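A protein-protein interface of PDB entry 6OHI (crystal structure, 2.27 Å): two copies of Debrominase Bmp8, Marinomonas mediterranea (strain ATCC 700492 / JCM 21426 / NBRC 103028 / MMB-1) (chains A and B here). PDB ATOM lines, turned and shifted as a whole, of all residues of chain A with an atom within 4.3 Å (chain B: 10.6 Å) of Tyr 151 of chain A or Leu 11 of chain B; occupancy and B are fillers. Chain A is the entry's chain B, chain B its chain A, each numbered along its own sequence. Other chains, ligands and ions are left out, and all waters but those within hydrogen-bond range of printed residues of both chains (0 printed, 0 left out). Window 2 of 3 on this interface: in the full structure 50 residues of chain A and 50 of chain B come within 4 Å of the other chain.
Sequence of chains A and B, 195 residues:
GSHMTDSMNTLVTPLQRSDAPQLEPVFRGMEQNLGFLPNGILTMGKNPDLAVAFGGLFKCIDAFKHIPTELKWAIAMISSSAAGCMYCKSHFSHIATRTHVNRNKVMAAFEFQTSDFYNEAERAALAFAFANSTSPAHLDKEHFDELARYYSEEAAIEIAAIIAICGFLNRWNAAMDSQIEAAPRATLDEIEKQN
No position is printed for both chains. Of the 7 pairs that touch across the chains among the printed residues, none has its exchanged pair printed and touching as well.
OD1 of Asn 9 of chain B lies within hydrogen-bond range of N of Leu 11 of chain B. ND2 of Asn 9 of chain B sits at hydrogen-bond distance from O of Val 12 of chain B (3.1 Å). O of Thr 13 of chain B is in hydrogen-bond range of NZ of Lys 46 of chain B (3.0 Å). OH of Tyr 151 of chain A is in hydrogen-bond range of O of Ala 121 of chain A. OG of Ser 152 of chain A sits at hydrogen-bond distance from N of Ala 155 of chain A (3.3 Å).
The backbone NH (N) of Thr 13 of chain B lies within hydrogen-bond range of the side-chain carboxylate (OE1) of Glu 153 of chain A (3.0 Å). OE1 of Glu 153 of chain A lies within salt-bridge range of NZ of Lys 46 of chain B (2.6 Å).
Among the printed residues, pairs that only touch across the chains: Glu 153 of chain A with Val 12 of chain B, Ala 156 of chain A with Leu 11 of chain B, Tyr 151 of chain A with Leu 11 of chain B, Glu 153 of chain A with Leu 11 of chain B and Ser 152 of chain A with Leu 11 of chain B.
Printed residues of chain A that touch a printed residue of chain B: Tyr 151, Ser 152, Glu 153 and Ala 156. Hydrophobic or aromatic side chains of chain B that line the printed part of chain A: Leu 11 and Val 12. Among the printed residues, 7 pairs touch across the chains. Among the printed residues, Asp or Glu carboxylates within 4 Å of a Lys or Arg side-chain nitrogen of the other chain: Glu 153 of chain A with Lys 46 of chain B.
Of the printed residues of chain B, Tyr 151 of chain A touches Leu 11 (3.6 Å). Leu 11 of chain B touches just these residues of chain A: Tyr 151, Ser 152, Glu 153 and Ala 156. No residue of chain B comes within 4 Å of Ala 121 of chain A. Ala 125 of chain A touches none of the printed residues of chain B. No residue of chain B comes within 4 Å of Ala 155 of chain A. Of the printed residues of chain A, Thr 13 of chain B touches Glu 153. Of the printed residues of chain B, Ala 156 of chain A touches Leu 11 (3.5 Å). Of the printed residues of chain A, Lys 46 of chain B touches Glu 153. Glu 122 of chain A touches none of the printed residues of chain B. Met 8 of chain B touches none of the printed residues of chain A. The nearest residue of chain B that does not touch Tyr 151 of chain A is Val 12 of chain B (7.9 Å). The nearest residue of chain A that does not touch Leu 11 of chain B is Ala 148 of chain A (4.03 Å). The nearest printed residue of chain B that does not touch Ala 156 of chain A is Val 12 of chain B (4.8 Å).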
ATOM      1  N   LEU A  71      12.895 -10.170   0.281  1.00  0.00           N
ATOM      2  CA  LEU A  71      13.076 -11.548  -0.127  1.00  0.00           C
ATOM      3  C   LEU A  71      14.570 -11.867  -0.279  1.00  0.00           C
ATOM      4  O   LEU A  71      15.011 -12.970   0.053  1.00  0.00           O
ATOM      5  CB  LEU A  71      12.335 -11.803  -1.441  1.00  0.00           C
ATOM      6  CG  LEU A  71      12.281 -13.274  -1.845  1.00  0.00           C
ATOM      7  CD1 LEU A  71      11.534 -14.079  -0.802  1.00  0.00           C
ATOM      8  CD2 LEU A  71      11.646 -13.471  -3.214  1.00  0.00           C
ATOM      9  N   ALA A 121       4.603 -17.925  -3.123  1.00  0.00           N
ATOM     10  CA  ALA A 121       5.711 -17.444  -3.952  1.00  0.00           C
ATOM     11  C   ALA A 121       6.984 -17.365  -3.107  1.00  0.00           C
ATOM     12  O   ALA A 121       8.039 -17.818  -3.523  1.00  0.00           O
ATOM     13  CB  ALA A 121       5.388 -16.096  -4.565  1.00  0.00           C
ATOM     14  N   GLU A 122       6.855 -16.777  -1.915  1.00  0.00           N
ATOM     15  CA  GLU A 122       7.961 -16.645  -0.993  1.00  0.00           C
ATOM     16  C   GLU A 122       8.444 -18.033  -0.551  1.00  0.00           C
ATOM     17  O   GLU A 122       9.648 -18.283  -0.498  1.00  0.00           O
ATOM     18  CB  GLU A 122       7.547 -15.770   0.190  1.00  0.00           C
ATOM     19  CG  GLU A 122       7.395 -14.310  -0.199  1.00  0.00           C
ATOM     20  CD  GLU A 122       6.686 -13.426   0.808  1.00  0.00           C
ATOM     21  OE1 GLU A 122       5.750 -13.909   1.496  1.00  0.00           O
ATOM     22  OE2 GLU A 122       7.028 -12.241   0.848  1.00  0.00           O
ATOM     23  N   ALA A 125      10.592 -19.853  -3.106  1.00  0.00           N
ATOM     24  CA  ALA A 125      11.949 -19.317  -3.174  1.00  0.00           C
ATOM     25  C   ALA A 125      12.770 -19.769  -1.959  1.00  0.00           C
ATOM     26  O   ALA A 125      13.945 -20.115  -2.101  1.00  0.00           O
ATOM     27  CB  ALA A 125      11.917 -17.810  -3.265  1.00  0.00           C
ATOM     28  N   LEU A 147       9.327 -23.175  -8.284  1.00  0.00           N
ATOM     29  CA  LEU A 147      10.030 -21.926  -8.600  1.00  0.00           C
ATOM     30  C   LEU A 147       9.528 -21.375  -9.941  1.00  0.00           C
ATOM     31  O   LEU A 147       9.267 -20.181 -10.058  1.00  0.00           O
ATOM     32  CB  LEU A 147      11.543 -22.154  -8.645  1.00  0.00           C
ATOM     33  CG  LEU A 147      12.386 -20.888  -8.496  1.00  0.00           C
ATOM     34  CD1 LEU A 147      12.349 -20.389  -7.061  1.00  0.00           C
ATOM     35  CD2 LEU A 147      13.821 -21.124  -8.957  1.00  0.00           C
ATOM     36  N   ALA A 148       9.400 -22.263 -10.937  1.00  0.00           N
ATOM     37  CA  ALA A 148       8.906 -21.907 -12.281  1.00  0.00           C
ATOM     38  C   ALA A 148       7.469 -21.374 -12.202  1.00  0.00           C
ATOM     39  O   ALA A 148       7.081 -20.522 -12.990  1.00  0.00           O
ATOM     40  CB  ALA A 148       8.993 -23.102 -13.204  1.00  0.00           C
ATOM     41  N   ARG A 149       6.693 -21.882 -11.241  1.00  0.00           N
ATOM     42  CA  ARG A 149       5.308 -21.490 -11.078  1.00  0.00           C
ATOM     43  C   ARG A 149       5.206 -20.015 -10.668  1.00  0.00           C
ATOM     44  O   ARG A 149       4.240 -19.349 -11.032  1.00  0.00           O
ATOM     45  CB  ARG A 149       4.628 -22.403 -10.053  1.00  0.00           C
ATOM     46  CG  ARG A 149       3.113 -22.292 -10.034  1.00  0.00           C
ATOM     47  CD  ARG A 149       2.439 -23.646  -9.919  1.00  0.00           C
ATOM     48  NE  ARG A 149       2.312 -24.079  -8.538  1.00  0.00           N
ATOM     49  CZ  ARG A 149       1.273 -23.799  -7.755  1.00  0.00           C
ATOM     50  NH1 ARG A 149       0.311 -22.994  -8.185  1.00  0.00           N
ATOM     51  NH2 ARG A 149       1.196 -24.332  -6.547  1.00  0.00           N
ATOM     52  N   TYR A 150       6.192 -19.502  -9.918  1.00  0.00           N
ATOM     53  CA  TYR A 150       6.044 -18.196  -9.270  1.00  0.00           C
ATOM     54  C   TYR A 150       7.121 -17.182  -9.682  1.00  0.00           C
ATOM     55  O   TYR A 150       7.046 -16.030  -9.251  1.00  0.00           O
ATOM     56  CB  TYR A 150       6.064 -18.365  -7.750  1.00  0.00           C
ATOM     57  CG  TYR A 150       4.893 -19.137  -7.199  1.00  0.00           C
ATOM     58  CD1 TYR A 150       3.621 -18.581  -7.156  1.00  0.00           C
ATOM     59  CD2 TYR A 150       5.060 -20.419  -6.701  1.00  0.00           C
ATOM     60  CE1 TYR A 150       2.543 -19.288  -6.646  1.00  0.00           C
ATOM     61  CE2 TYR A 150       3.993 -21.136  -6.183  1.00  0.00           C
ATOM     62  CZ  TYR A 150       2.732 -20.568  -6.154  1.00  0.00           C
ATOM     63  OH  TYR A 150       1.694 -21.284  -5.638  1.00  0.00           O
ATOM     64  N   TYR A 151       8.105 -17.579 -10.500  1.00  0.00           N
ATOM     65  CA  TYR A 151       9.222 -16.669 -10.814  1.00  0.00           C
ATOM     66  C   TYR A 151       9.662 -16.784 -12.278  1.00  0.00           C
ATOM     67  O   TYR A 151       9.690 -17.873 -12.860  1.00  0.00           O
ATOM     68  CB  TYR A 151      10.413 -16.946  -9.896  1.00  0.00           C
ATOM     69  CG  TYR A 151      10.149 -16.614  -8.452  1.00  0.00           C
ATOM     70  CD1 TYR A 151      10.115 -15.298  -8.023  1.00  0.00           C
ATOM     71  CD2 TYR A 151       9.912 -17.608  -7.514  1.00  0.00           C
ATOM     72  CE1 TYR A 151       9.858 -14.976  -6.701  1.00  0.00           C
ATOM     73  CE2 TYR A 151       9.669 -17.303  -6.184  1.00  0.00           C
ATOM     74  CZ  TYR A 151       9.643 -15.981  -5.773  1.00  0.00           C
ATOM     75  OH  TYR A 151       9.398 -15.659  -4.466  1.00  0.00           O
ATOM     76  N   SER A 152      10.041 -15.630 -12.843  1.00  0.00           N
ATOM     77  CA  SER A 152      10.650 -15.543 -14.166  1.00  0.00           C
ATOM     78  C   SER A 152      12.076 -16.101 -14.113  1.00  0.00           C
ATOM     79  O   SER A 152      12.667 -16.216 -13.032  1.00  0.00           O
ATOM     80  CB  SER A 152      10.647 -14.117 -14.680  1.00  0.00           C
ATOM     81  OG  SER A 152      11.412 -13.266 -13.835  1.00  0.00           O
ATOM     82  N   GLU A 153      12.616 -16.420 -15.295  1.00  0.00           N
ATOM     83  CA  GLU A 153      14.013 -16.806 -15.470  1.00  0.00           C
ATOM     84  C   GLU A 153      14.938 -15.769 -14.810  1.00  0.00           C
ATOM     85  O   GLU A 153      15.904 -16.137 -14.129  1.00  0.00           O
ATOM     86  CB  GLU A 153      14.312 -16.954 -16.961  1.00  0.00           C
ATOM     87  CG  GLU A 153      15.761 -17.262 -17.280  1.00  0.00           C
ATOM     88  CD  GLU A 153      15.988 -17.715 -18.711  1.00  0.00           C
ATOM     89  OE1 GLU A 153      17.002 -18.390 -18.974  1.00  0.00           O
ATOM     90  OE2 GLU A 153      15.145 -17.398 -19.564  1.00  0.00           O
ATOM     91  N   ALA A 155      14.326 -13.668 -12.368  1.00  0.00           N
ATOM     92  CA  ALA A 155      14.171 -13.751 -10.927  1.00  0.00           C
ATOM     93  C   ALA A 155      14.882 -14.999 -10.389  1.00  0.00           C
ATOM     94  O   ALA A 155      15.557 -14.931  -9.370  1.00  0.00           O
ATOM     95  CB  ALA A 155      12.704 -13.762 -10.567  1.00  0.00           C
ATOM     96  N   ALA A 156      14.701 -16.133 -11.071  1.00  0.00           N
ATOM     97  CA  ALA A 156      15.279 -17.405 -10.637  1.00  0.00           C
ATOM     98  C   ALA A 156      16.809 -17.291 -10.563  1.00  0.00           C
ATOM     99  O   ALA A 156      17.433 -17.812  -9.631  1.00  0.00           O
ATOM    100  CB  ALA A 156      14.850 -18.516 -11.562  1.00  0.00           C
ATOM    101  N   ILE A 159      17.783 -15.317  -7.453  1.00  0.00           N
ATOM    102  CA  ILE A 159      17.584 -16.178  -6.290  1.00  0.00           C
ATOM    103  C   ILE A 159      18.790 -17.123  -6.171  1.00  0.00           C
ATOM    104  O   ILE A 159      19.452 -17.158  -5.129  1.00  0.00           O
ATOM    105  CB  ILE A 159      16.241 -16.934  -6.401  1.00  0.00           C
ATOM    106  CG1 ILE A 159      15.061 -15.973  -6.238  1.00  0.00           C
ATOM    107  CG2 ILE A 159      16.161 -18.100  -5.417  1.00  0.00           C
ATOM    108  CD1 ILE A 159      13.723 -16.566  -6.610  1.00  0.00           C
ATOM    109  N   ASP B   6      17.044 -35.727 -18.534  1.00  0.00           N
ATOM    110  CA  ASP B   6      17.717 -34.399 -18.634  1.00  0.00           C
ATOM    111  C   ASP B   6      17.639 -33.706 -17.263  1.00  0.00           C
ATOM    112  O   ASP B   6      17.551 -34.354 -16.229  1.00  0.00           O
ATOM    113  CB  ASP B   6      17.109 -33.575 -19.779  1.00  0.00           C
ATOM    114  CG  ASP B   6      18.007 -32.468 -20.321  1.00  0.00           C
ATOM    115  OD1 ASP B   6      19.232 -32.695 -20.421  1.00  0.00           O
ATOM    116  OD2 ASP B   6      17.477 -31.373 -20.625  1.00  0.00           O
ATOM    117  N   SER B   7      17.677 -32.373 -17.281  1.00  0.00           N
ATOM    118  CA  SER B   7      17.720 -31.518 -16.105  1.00  0.00           C
ATOM    119  C   SER B   7      16.306 -31.340 -15.536  1.00  0.00           C
ATOM    120  O   SER B   7      15.320 -31.326 -16.284  1.00  0.00           O
ATOM    121  CB  SER B   7      18.339 -30.190 -16.494  1.00  0.00           C
ATOM    122  OG  SER B   7      18.409 -29.281 -15.407  1.00  0.00           O
ATOM    123  N   MET B   8      16.225 -31.178 -14.210  1.00  0.00           N
ATOM    124  CA  MET B   8      14.975 -30.867 -13.527  1.00  0.00           C
ATOM    125  C   MET B   8      14.601 -29.400 -13.757  1.00  0.00           C
ATOM    126  O   MET B   8      13.463 -29.010 -13.536  1.00  0.00           O
ATOM    127  CB  MET B   8      15.107 -31.101 -12.022  1.00  0.00           C
ATOM    128  CG  MET B   8      15.370 -32.546 -11.648  1.00  0.00           C
ATOM    129  SD  MET B   8      15.542 -32.728  -9.857  1.00  0.00           S
ATOM    130  CE  MET B   8      17.212 -32.123  -9.609  1.00  0.00           C
ATOM    131  N   ASN B   9      15.585 -28.606 -14.186  1.00  0.00           N
ATOM    132  CA  ASN B   9      15.460 -27.174 -14.399  1.00  0.00           C
ATOM    133  C   ASN B   9      15.194 -26.894 -15.885  1.00  0.00           C
ATOM    134  O   ASN B   9      16.075 -27.107 -16.723  1.00  0.00           O
ATOM    135  CB  ASN B   9      16.722 -26.454 -13.919  1.00  0.00           C
ATOM    136  CG  ASN B   9      16.935 -25.119 -14.596  1.00  0.00           C
ATOM    137  OD1 ASN B   9      16.017 -24.302 -14.671  1.00  0.00           O
ATOM    138  ND2 ASN B   9      18.140 -24.900 -15.099  1.00  0.00           N
ATOM    139  N   THR B  10      13.982 -26.409 -16.188  1.00  0.00           N
ATOM    140  CA  THR B  10      13.579 -26.038 -17.556  1.00  0.00           C
ATOM    141  C   THR B  10      13.360 -24.520 -17.676  1.00  0.00           C
ATOM    142  O   THR B  10      13.230 -24.004 -18.790  1.00  0.00           O
ATOM    143  CB  THR B  10      12.325 -26.816 -17.976  1.00  0.00           C
ATOM    144  OG1 THR B  10      11.319 -26.594 -16.985  1.00  0.00           O
ATOM    145  CG2 THR B  10      12.587 -28.301 -18.133  1.00  0.00           C
ATOM    146  N   LEU B  11      13.360 -23.815 -16.540  1.00  0.00           N
ATOM    147  CA  LEU B  11      13.055 -22.388 -16.482  1.00  0.00           C
ATOM    148  C   LEU B  11      14.227 -21.553 -17.013  1.00  0.00           C
ATOM    149  O   LEU B  11      14.013 -20.607 -17.759  1.00  0.00           O
ATOM    150  CB  LEU B  11      12.745 -21.986 -15.036  1.00  0.00           C
ATOM    151  CG  LEU B  11      12.565 -20.484 -14.819  1.00  0.00           C
ATOM    152  CD1 LEU B  11      11.394 -19.958 -15.639  1.00  0.00           C
ATOM    153  CD2 LEU B  11      12.380 -20.157 -13.345  1.00  0.00           C
ATOM    154  N   VAL B  12      15.447 -21.865 -16.566  1.00  0.00           N
ATOM    155  CA  VAL B  12      16.601 -21.005 -16.816  1.00  0.00           C
ATOM    156  C   VAL B  12      17.586 -21.751 -17.724  1.00  0.00           C
ATOM    157  O   VAL B  12      18.279 -22.661 -17.291  1.00  0.00           O
ATOM    158  CB  VAL B  12      17.256 -20.493 -15.517  1.00  0.00           C
ATOM    159  CG1 VAL B  12      17.308 -21.549 -14.430  1.00  0.00           C
ATOM    160  CG2 VAL B  12      18.645 -19.919 -15.761  1.00  0.00           C
ATOM    161  N   THR B  13      17.631 -21.312 -18.986  1.00  0.00           N
ATOM    162  CA  THR B  13      18.359 -21.957 -20.056  1.00  0.00           C
ATOM    163  C   THR B  13      19.573 -21.112 -20.430  1.00  0.00           C
ATOM    164  O   THR B  13      19.569 -19.891 -20.263  1.00  0.00           O
ATOM    165  CB  THR B  13      17.438 -22.174 -21.263  1.00  0.00           C
ATOM    166  OG1 THR B  13      16.955 -20.897 -21.675  1.00  0.00           O
ATOM    167  CG2 THR B  13      16.265 -23.080 -20.956  1.00  0.00           C
ATOM    168  N   PRO B  14      20.654 -21.737 -20.952  1.00  0.00           N
ATOM    169  CA  PRO B  14      21.826 -20.990 -21.410  1.00  0.00           C
ATOM    170  C   PRO B  14      21.520 -20.187 -22.682  1.00  0.00           C
ATOM    171  O   PRO B  14      20.686 -20.603 -23.500  1.00  0.00           O
ATOM    172  CB  PRO B  14      22.872 -22.081 -21.689  1.00  0.00           C
ATOM    173  CG  PRO B  14      22.037 -23.315 -21.997  1.00  0.00           C
ATOM    174  CD  PRO B  14      20.802 -23.192 -21.127  1.00  0.00           C
ATOM    175  N   LEU B  15      22.190 -19.040 -22.832  1.00  0.00           N
ATOM    176  CA  LEU B  15      22.220 -18.346 -24.117  1.00  0.00           C
ATOM    177  C   LEU B  15      23.304 -19.012 -24.981  1.00  0.00           C
ATOM    178  O   LEU B  15      24.103 -19.789 -24.471  1.00  0.00           O
ATOM    179  CB  LEU B  15      22.443 -16.838 -23.916  1.00  0.00           C
ATOM    180  CG  LEU B  15      23.398 -16.407 -22.799  1.00  0.00           C
ATOM    181  CD1 LEU B  15      24.798 -16.940 -23.045  1.00  0.00           C
ATOM    182  CD2 LEU B  15      23.440 -14.892 -22.655  1.00  0.00           C
ATOM    183  N   THR B  43      24.358 -19.678 -18.640  1.00  0.00           N
ATOM    184  CA  THR B  43      23.105 -19.290 -17.959  1.00  0.00           C
ATOM    185  C   THR B  43      23.367 -18.032 -17.120  1.00  0.00           C
ATOM    186  O   THR B  43      22.567 -17.097 -17.128  1.00  0.00           O
ATOM    187  CB  THR B  43      22.522 -20.418 -17.096  1.00  0.00           C
ATOM    188  OG1 THR B  43      23.523 -20.840 -16.173  1.00  0.00           O
ATOM    189  CG2 THR B  43      22.070 -21.625 -17.887  1.00  0.00           C
ATOM    190  N   LYS B  46      23.170 -14.324 -18.600  1.00  0.00           N
ATOM    191  CA  LYS B  46      21.922 -13.581 -18.777  1.00  0.00           C
ATOM    192  C   LYS B  46      21.783 -12.467 -17.728  1.00  0.00           C
ATOM    193  O   LYS B  46      20.887 -11.627 -17.838  1.00  0.00           O
ATOM    194  CB  LYS B  46      20.727 -14.536 -18.717  1.00  0.00           C
ATOM    195  CG  LYS B  46      20.617 -15.487 -19.897  1.00  0.00           C
ATOM    196  CD  LYS B  46      19.262 -16.156 -20.009  1.00  0.00           C
ATOM    197  CE  LYS B  46      19.092 -16.909 -21.311  1.00  0.00           C
ATOM    198  NZ  LYS B  46      17.818 -17.664 -21.337  1.00  0.00           N
ATOM    199  N   ALA B 175      21.669 -25.365  -8.351  1.00  0.00           N
ATOM    200  CA  ALA B 175      20.500 -24.529  -8.663  1.00  0.00           C
ATOM    201  C   ALA B 175      20.131 -24.598 -10.158  1.00  0.00           C
ATOM    202  O   ALA B 175      18.973 -24.475 -10.503  1.00  0.00           O
ATOM    203  CB  ALA B 175      20.752 -23.112  -8.220  1.00  0.00           C
ATOM    204  N   MET B 176      21.115 -24.807 -11.038  1.00  0.00           N
ATOM    205  CA  MET B 176      20.874 -24.974 -12.476  1.00  0.00           C
ATOM    206  C   MET B 176      20.584 -26.450 -12.806  1.00  0.00           C
ATOM    207  O   MET B 176      20.088 -26.758 -13.893  1.00  0.00           O
ATOM    208  CB  MET B 176      22.093 -24.517 -13.282  1.00  0.00           C
ATOM    209  CG  MET B 176      22.511 -23.084 -13.013  1.00  0.00           C
ATOM    210  SD  MET B 176      21.282 -21.887 -13.567  1.00  0.00           S
ATOM    211  CE  MET B 176      20.505 -21.418 -12.026  1.00  0.00           C
ATOM    212  N   ASP B 177      20.890 -27.348 -11.859  1.00  0.00           N
ATOM    213  CA  ASP B 177      20.872 -28.804 -12.046  1.00  0.00           C
ATOM    214  C   ASP B 177      21.705 -29.165 -13.278  1.00  0.00           C
ATOM    215  O   ASP B 177      21.273 -29.943 -14.129  1.00  0.00           O
ATOM    216  CB  ASP B 177      19.446 -29.360 -12.146  1.00  0.00           C
ATOM    217  CG  ASP B 177      19.359 -30.851 -11.853  1.00  0.00           C
ATOM    218  OD1 ASP B 177      20.100 -31.304 -10.956  1.00  0.00           O
ATOM    219  OD2 ASP B 177      18.556 -31.546 -12.521  1.00  0.00           O
